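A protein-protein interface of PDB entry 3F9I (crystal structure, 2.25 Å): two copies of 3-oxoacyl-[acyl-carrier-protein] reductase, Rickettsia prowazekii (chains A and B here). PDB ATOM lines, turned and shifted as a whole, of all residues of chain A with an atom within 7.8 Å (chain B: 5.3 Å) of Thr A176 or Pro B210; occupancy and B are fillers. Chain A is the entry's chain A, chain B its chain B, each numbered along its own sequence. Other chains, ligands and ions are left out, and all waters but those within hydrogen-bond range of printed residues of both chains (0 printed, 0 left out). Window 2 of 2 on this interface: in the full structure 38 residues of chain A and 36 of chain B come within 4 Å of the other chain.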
ATOM      1  N   ILE A 131      25.109  12.431   2.948  1.00  0.00           N
ATOM      2  CA  ILE A 131      26.510  12.028   3.110  1.00  0.00           C
ATOM      3  C   ILE A 131      26.795  11.603   4.554  1.00  0.00           C
ATOM      4  O   ILE A 131      27.531  10.650   4.779  1.00  0.00           O
ATOM      5  CB  ILE A 131      27.502  13.177   2.701  1.00  0.00           C
ATOM      6  CG1 ILE A 131      27.523  13.359   1.188  1.00  0.00           C
ATOM      7  CG2 ILE A 131      28.919  12.863   3.091  1.00  0.00           C
ATOM      8  CD1 ILE A 131      27.225  12.104   0.446  1.00  0.00           C
ATOM      9  N   ARG A 134      25.725   8.118   5.011  1.00  0.00           N
ATOM     10  CA  ARG A 134      26.084   7.184   3.911  1.00  0.00           C
ATOM     11  C   ARG A 134      24.863   6.427   3.367  1.00  0.00           C
ATOM     12  O   ARG A 134      24.925   5.263   3.096  1.00  0.00           O
ATOM     13  CB  ARG A 134      27.143   6.161   4.344  1.00  0.00           C
ATOM     14  CG  ARG A 134      28.559   6.698   4.474  1.00  0.00           C
ATOM     15  CD  ARG A 134      29.599   5.544   4.755  1.00  0.00           C
ATOM     16  NE  ARG A 134      29.410   4.436   3.801  1.00  0.00           N
ATOM     17  CZ  ARG A 134      29.888   4.410   2.550  1.00  0.00           C
ATOM     18  NH1 ARG A 134      30.650   5.398   2.073  1.00  0.00           N
ATOM     19  NH2 ARG A 134      29.608   3.376   1.771  1.00  0.00           N
ATOM     20  N   LYS A 168      22.531  12.329 -13.560  1.00  0.00           N
ATOM     21  CA  LYS A 168      23.739  11.524 -13.853  1.00  0.00           C
ATOM     22  C   LYS A 168      25.003  12.084 -13.215  1.00  0.00           C
ATOM     23  O   LYS A 168      25.769  11.382 -12.612  1.00  0.00           O
ATOM     24  CB  LYS A 168      23.973  11.430 -15.347  1.00  0.00           C
ATOM     25  CG  LYS A 168      22.862  10.775 -16.110  1.00  0.00           C
ATOM     26  CD  LYS A 168      23.125  10.903 -17.617  1.00  0.00           C
ATOM     27  CE  LYS A 168      22.059  10.130 -18.428  1.00  0.00           C
ATOM     28  NZ  LYS A 168      21.772  10.673 -19.774  1.00  0.00           N
ATOM     29  N   SER A 171      24.875  11.628  -9.554  1.00  0.00           N
ATOM     30  CA  SER A 171      24.871  10.216  -9.310  1.00  0.00           C
ATOM     31  C   SER A 171      26.283   9.696  -9.143  1.00  0.00           C
ATOM     32  O   SER A 171      26.593   8.974  -8.197  1.00  0.00           O
ATOM     33  CB  SER A 171      24.191   9.508 -10.487  1.00  0.00           C
ATOM     34  OG  SER A 171      24.500   8.150 -10.513  1.00  0.00           O
ATOM     35  N   TYR A 172      27.122  10.035 -10.107  1.00  0.00           N
ATOM     36  CA  TYR A 172      28.533   9.651 -10.092  1.00  0.00           C
ATOM     37  C   TYR A 172      29.216  10.198  -8.806  1.00  0.00           C
ATOM     38  O   TYR A 172      29.909   9.485  -8.086  1.00  0.00           O
ATOM     39  CB  TYR A 172      29.185  10.164 -11.378  1.00  0.00           C
ATOM     40  CG  TYR A 172      30.594   9.701 -11.626  1.00  0.00           C
ATOM     41  CD1 TYR A 172      30.860   8.596 -12.448  1.00  0.00           C
ATOM     42  CD2 TYR A 172      31.693  10.396 -11.064  1.00  0.00           C
ATOM     43  CE1 TYR A 172      32.194   8.187 -12.694  1.00  0.00           C
ATOM     44  CE2 TYR A 172      33.002   9.986 -11.287  1.00  0.00           C
ATOM     45  CZ  TYR A 172      33.250   8.894 -12.103  1.00  0.00           C
ATOM     46  OH  TYR A 172      34.555   8.513 -12.313  1.00  0.00           O
ATOM     47  N   GLU A 173      28.925  11.446  -8.478  1.00  0.00           N
ATOM     48  CA  GLU A 173      29.540  12.114  -7.336  1.00  0.00           C
ATOM     49  C   GLU A 173      29.287  11.537  -5.911  1.00  0.00           C
ATOM     50  O   GLU A 173      30.119  11.708  -5.009  1.00  0.00           O
ATOM     51  CB  GLU A 173      29.072  13.553  -7.400  1.00  0.00           C
ATOM     52  CG  GLU A 173      29.411  14.422  -6.226  1.00  0.00           C
ATOM     53  CD  GLU A 173      28.952  15.826  -6.480  1.00  0.00           C
ATOM     54  OE1 GLU A 173      29.020  16.232  -7.664  1.00  0.00           O
ATOM     55  OE2 GLU A 173      28.500  16.507  -5.523  1.00  0.00           O
ATOM     56  N   VAL A 174      28.130  10.911  -5.702  1.00  0.00           N
ATOM     57  CA  VAL A 174      27.727  10.436  -4.390  1.00  0.00           C
ATOM     58  C   VAL A 174      27.713   8.930  -4.351  1.00  0.00           C
ATOM     59  O   VAL A 174      27.359   8.338  -3.330  1.00  0.00           O
ATOM     60  CB  VAL A 174      26.298  10.976  -3.967  1.00  0.00           C
ATOM     61  CG1 VAL A 174      26.309  12.489  -3.812  1.00  0.00           C
ATOM     62  CG2 VAL A 174      25.230  10.554  -4.939  1.00  0.00           C
ATOM     63  N   ALA A 175      28.096   8.303  -5.457  1.00  0.00           N
ATOM     64  CA  ALA A 175      27.942   6.858  -5.627  1.00  0.00           C
ATOM     65  C   ALA A 175      28.620   5.982  -4.546  1.00  0.00           C
ATOM     66  O   ALA A 175      28.045   4.975  -4.099  1.00  0.00           O
ATOM     67  CB  ALA A 175      28.417   6.454  -7.023  1.00  0.00           C
ATOM     68  N   THR A 176      29.834   6.334  -4.138  1.00  0.00           N
ATOM     69  CA  THR A 176      30.523   5.532  -3.120  1.00  0.00           C
ATOM     70  C   THR A 176      29.998   5.779  -1.723  1.00  0.00           C
ATOM     71  O   THR A 176      30.319   5.044  -0.799  1.00  0.00           O
ATOM     72  CB  THR A 176      32.011   5.780  -3.120  1.00  0.00           C
ATOM     73  OG1 THR A 176      32.254   7.197  -3.097  1.00  0.00           O
ATOM     74  CG2 THR A 176      32.604   5.128  -4.354  1.00  0.00           C
ATOM     75  N   ARG A 177      29.132   6.764  -1.578  1.00  0.00           N
ATOM     76  CA  ARG A 177      28.623   7.119  -0.287  1.00  0.00           C
ATOM     77  C   ARG A 177      27.201   6.708  -0.090  1.00  0.00           C
ATOM     78  O   ARG A 177      26.495   7.323   0.680  1.00  0.00           O
ATOM     79  CB  ARG A 177      28.802   8.610  -0.080  1.00  0.00           C
ATOM     80  CG  ARG A 177      30.215   8.909   0.335  1.00  0.00           C
ATOM     81  CD  ARG A 177      30.446  10.374   0.335  1.00  0.00           C
ATOM     82  NE  ARG A 177      30.441  10.890  -1.024  1.00  0.00           N
ATOM     83  CZ  ARG A 177      30.650  12.162  -1.328  1.00  0.00           C
ATOM     84  NH1 ARG A 177      30.865  13.051  -0.359  1.00  0.00           N
ATOM     85  NH2 ARG A 177      30.631  12.554  -2.595  1.00  0.00           N
ATOM     86  N   GLY A 178      26.775   5.652  -0.774  1.00  0.00           N
ATOM     87  CA  GLY A 178      25.512   5.014  -0.446  1.00  0.00           C
ATOM     88  C   GLY A 178      24.230   5.766  -0.807  1.00  0.00           C
ATOM     89  O   GLY A 178      23.123   5.391  -0.370  1.00  0.00           O
ATOM     90  N   ILE A 179      24.388   6.798  -1.618  1.00  0.00           N
ATOM     91  CA  ILE A 179      23.283   7.604  -2.112  1.00  0.00           C
ATOM     92  C   ILE A 179      23.081   7.265  -3.591  1.00  0.00           C
ATOM     93  O   ILE A 179      24.054   7.233  -4.347  1.00  0.00           O
ATOM     94  CB  ILE A 179      23.653   9.077  -1.995  1.00  0.00           C
ATOM     95  CG1 ILE A 179      23.826   9.468  -0.533  1.00  0.00           C
ATOM     96  CG2 ILE A 179      22.587   9.967  -2.657  1.00  0.00           C
ATOM     97  CD1 ILE A 179      24.634  10.752  -0.336  1.00  0.00           C
ATOM     98  N   TYR A 234      21.246  -0.726  -6.349  1.00  0.00           N
ATOM     99  CA  TYR A 234      22.297  -0.790  -7.359  1.00  0.00           C
ATOM    100  C   TYR A 234      21.912   0.009  -8.614  1.00  0.00           C
ATOM    101  O   TYR A 234      22.595  -0.066  -9.623  1.00  0.00           O
ATOM    102  CB  TYR A 234      22.587  -2.255  -7.735  1.00  0.00           C
ATOM    103  CG  TYR A 234      24.003  -2.482  -8.259  1.00  0.00           C
ATOM    104  CD1 TYR A 234      25.099  -2.106  -7.512  1.00  0.00           C
ATOM    105  CD2 TYR A 234      24.237  -3.098  -9.477  1.00  0.00           C
ATOM    106  CE1 TYR A 234      26.366  -2.320  -7.957  1.00  0.00           C
ATOM    107  CE2 TYR A 234      25.526  -3.322  -9.941  1.00  0.00           C
ATOM    108  CZ  TYR A 234      26.587  -2.929  -9.174  1.00  0.00           C
ATOM    109  OH  TYR A 234      27.890  -3.119  -9.594  1.00  0.00           O
ATOM    110  N   THR A 236      21.572   3.612 -10.049  1.00  0.00           N
ATOM    111  CA  THR A 236      21.836   5.040  -9.908  1.00  0.00           C
ATOM    112  C   THR A 236      22.186   5.662 -11.277  1.00  0.00           C
ATOM    113  O   THR A 236      22.654   4.944 -12.166  1.00  0.00           O
ATOM    114  CB  THR A 236      22.935   5.323  -8.887  1.00  0.00           C
ATOM    115  OG1 THR A 236      22.891   6.720  -8.534  1.00  0.00           O
ATOM    116  CG2 THR A 236      24.337   4.908  -9.426  1.00  0.00           C
ATOM    117  N   VAL B 206      36.059  -2.967 -10.519  1.00  0.00           N
ATOM    118  CA  VAL B 206      35.422  -2.102  -9.532  1.00  0.00           C
ATOM    119  C   VAL B 206      35.712  -0.614  -9.833  1.00  0.00           C
ATOM    120  O   VAL B 206      34.900   0.249  -9.497  1.00  0.00           O
ATOM    121  CB  VAL B 206      35.794  -2.508  -8.058  1.00  0.00           C
ATOM    122  CG1 VAL B 206      35.276  -1.501  -7.048  1.00  0.00           C
ATOM    123  CG2 VAL B 206      35.234  -3.886  -7.715  1.00  0.00           C
ATOM    124  N   GLN B 207      36.830  -0.305 -10.495  1.00  0.00           N
ATOM    125  CA  GLN B 207      37.067   1.072 -10.972  1.00  0.00           C
ATOM    126  C   GLN B 207      36.041   1.490 -12.060  1.00  0.00           C
ATOM    127  O   GLN B 207      35.676   2.636 -12.145  1.00  0.00           O
ATOM    128  CB  GLN B 207      38.524   1.285 -11.432  1.00  0.00           C
ATOM    129  N   LYS B 208      35.517   0.560 -12.837  1.00  0.00           N
ATOM    130  CA  LYS B 208      34.433   0.878 -13.799  1.00  0.00           C
ATOM    131  C   LYS B 208      33.046   1.262 -13.189  1.00  0.00           C
ATOM    132  O   LYS B 208      32.142   1.673 -13.910  1.00  0.00           O
ATOM    133  CB  LYS B 208      34.182  -0.317 -14.722  1.00  0.00           C
ATOM    134  CG  LYS B 208      35.395  -0.909 -15.426  1.00  0.00           C
ATOM    135  CD  LYS B 208      36.142   0.112 -16.244  1.00  0.00           C
ATOM    136  CE  LYS B 208      37.056  -0.572 -17.290  1.00  0.00           C
ATOM    137  NZ  LYS B 208      37.545   0.425 -18.315  1.00  0.00           N
ATOM    138  N   ILE B 209      32.882   1.094 -11.883  1.00  0.00           N
ATOM    139  CA  ILE B 209      31.575   1.126 -11.261  1.00  0.00           C
ATOM    140  C   ILE B 209      31.553   2.216 -10.230  1.00  0.00           C
ATOM    141  O   ILE B 209      32.180   2.091  -9.198  1.00  0.00           O
ATOM    142  CB  ILE B 209      31.278  -0.200 -10.542  1.00  0.00           C
ATOM    143  CG1 ILE B 209      31.429  -1.376 -11.519  1.00  0.00           C
ATOM    144  CG2 ILE B 209      29.884  -0.167  -9.885  1.00  0.00           C
ATOM    145  CD1 ILE B 209      31.289  -2.690 -10.861  1.00  0.00           C
ATOM    146  N   PRO B 210      30.829   3.302 -10.503  1.00  0.00           N
ATOM    147  CA  PRO B 210      30.721   4.402  -9.563  1.00  0.00           C
ATOM    148  C   PRO B 210      30.391   4.001  -8.146  1.00  0.00           C
ATOM    149  O   PRO B 210      30.882   4.628  -7.209  1.00  0.00           O
ATOM    150  CB  PRO B 210      29.588   5.232 -10.159  1.00  0.00           C
ATOM    151  CG  PRO B 210      29.824   5.103 -11.599  1.00  0.00           C
ATOM    152  CD  PRO B 210      30.250   3.667 -11.802  1.00  0.00           C
ATOM    153  N   LEU B 211      29.524   3.018  -7.986  1.00  0.00           N
ATOM    154  CA  LEU B 211      29.095   2.570  -6.634  1.00  0.00           C
ATOM    155  C   LEU B 211      30.231   1.902  -5.884  1.00  0.00           C
ATOM    156  O   LEU B 211      30.177   1.738  -4.673  1.00  0.00           O
ATOM    157  CB  LEU B 211      27.926   1.573  -6.735  1.00  0.00           C
ATOM    158  CG  LEU B 211      26.668   1.924  -5.953  1.00  0.00           C
ATOM    159  CD1 LEU B 211      26.006   3.115  -6.605  1.00  0.00           C
ATOM    160  CD2 LEU B 211      25.730   0.690  -5.878  1.00  0.00           C
ATOM    161  N   GLY B 212      31.257   1.509  -6.626  1.00  0.00           N
ATOM    162  CA  GLY B 212      32.441   0.889  -6.071  1.00  0.00           C
ATOM    163  C   GLY B 212      32.160  -0.499  -5.541  1.00  0.00           C
ATOM    164  O   GLY B 212      32.793  -0.941  -4.598  1.00  0.00           O
ATOM    165  N   GLY B 244      25.136  -0.138 -10.957  1.00  0.00           N
ATOM    166  CA  GLY B 244      25.906   0.672 -10.035  1.00  0.00           C
ATOM    167  C   GLY B 244      26.393   1.969 -10.643  1.00  0.00           C
ATOM    168  O   GLY B 244      27.369   2.542 -10.176  1.00  0.00           O
ATOM    169  N   GLY B 245      25.718   2.411 -11.698  1.00  0.00           N
ATOM    170  CA  GLY B 245      25.970   3.701 -12.310  1.00  0.00           C
ATOM    171  C   GLY B 245      27.051   3.649 -13.338  1.00  0.00           C
ATOM    172  O   GLY B 245      27.469   4.676 -13.816  1.00  0.00           O
ATOM    173  N   MET B 246      27.489   2.452 -13.715  1.00  0.00           N
ATOM    174  CA  MET B 246      28.653   2.329 -14.580  1.00  0.00           C
ATOM    175  C   MET B 246      28.299   2.769 -15.983  1.00  0.00           C
ATOM    176  O   MET B 246      29.166   3.157 -16.767  1.00  0.00           O
ATOM    177  CB  MET B 246      29.194   0.910 -14.579  1.00  0.00           C
ATOM    178  CG  MET B 246      28.419  -0.076 -15.367  1.00  0.00           C
ATOM    179  SD  MET B 246      29.450  -1.497 -15.802  1.00  0.00           S
ATOM    180  CE  MET B 246      28.405  -2.145 -17.083  1.00  0.00           C
ATOM    181  N   MET B 248      24.912   5.041 -17.547  1.00  0.00           N
ATOM    182  CA  MET B 248      23.725   5.849 -17.268  1.00  0.00           C
ATOM    183  C   MET B 248      22.930   6.162 -18.558  1.00  0.00           C
ATOM    184  O   MET B 248      23.383   6.966 -19.392  1.00  0.00           O
ATOM    185  CB  MET B 248      24.151   7.139 -16.535  1.00  0.00           C
ATOM    186  CG  MET B 248      24.846   6.846 -15.209  1.00  0.00           C
ATOM    187  SD  MET B 248      25.735   8.191 -14.413  1.00  0.00           S
ATOM    188  CE  MET B 248      26.236   7.420 -12.868  1.00  0.00           C
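O of Tyr A234 is in hydrogen-bond range of N of Gly B244, at 2.9 Å.
O of Lys A168 sits close to SD of Met B248, 3.7 Å away.
The backbone carbonyl oxygen (O) of Gly B244 is in hydrogen-bond range of the backbone NH (N) of Leu B211, 3.1 Å away.
OG of Ser A171 lies within hydrogen-bond range of OG1 of Thr A236, at 2.9 Å.
The guanidinium group of Arg A134 lies within hydrogen-bond range of the backbone carbonyl oxygen of Thr A176, at 2.9 Å.
Among the printed residues, merely in contact across the chains: Ser A171 with Met B248 (3.0 Å), Ala A175 with Pro B210 (3.1 Å), Tyr A234 with Leu B211 (3.3 Å), Thr A176 with Pro B210 (3.4 Å), Thr A236 with Gly B245 (3.5 Å), Tyr A234 with Ile B209 (3.6 Å), Ala A175 with Leu B211 (3.6 Å), Thr A236 with Leu B211 (3.7 Å), Tyr A172 with Pro B210 (3.7 Å), Thr A236 with Gly B244 (3.8 Å) and Tyr A172 with Met B248 (3.9 Å).
Thr A176 touches just one residue of chain B: Pro B210.
Of the printed residues of chain A, Pro B210 touches Tyr A172 (3.7 Å), Ala A175 (3.1 Å) and Thr A176 (3.4 Å).
Printed residues of chain A within 4 Å of Leu B211: Ala A175, Tyr A234 and Thr A236.
Of the printed residues of chain A, Ile B209 touches Tyr A234.
Val A174 touches none of the printed residues of chain B.
The nearest residue of chain B that does not touch Thr A176 is Leu B211 (4.1 Å).
The nearest printed residue of chain A that does not touch Gly B245 is Tyr A234 (4.5 Å).
Of the 11 printed residues of chain B, 6 touch a printed residue of chain A.
Among the printed residues, no Asp or Glu carboxylate lies within 4 Å of a Lys or Arg side-chain nitrogen of the other chain.
No position is printed for both chains.
Of the 13 pairs that touch across the chains among the printed residues, none has its exchanged pair printed and touching as well.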
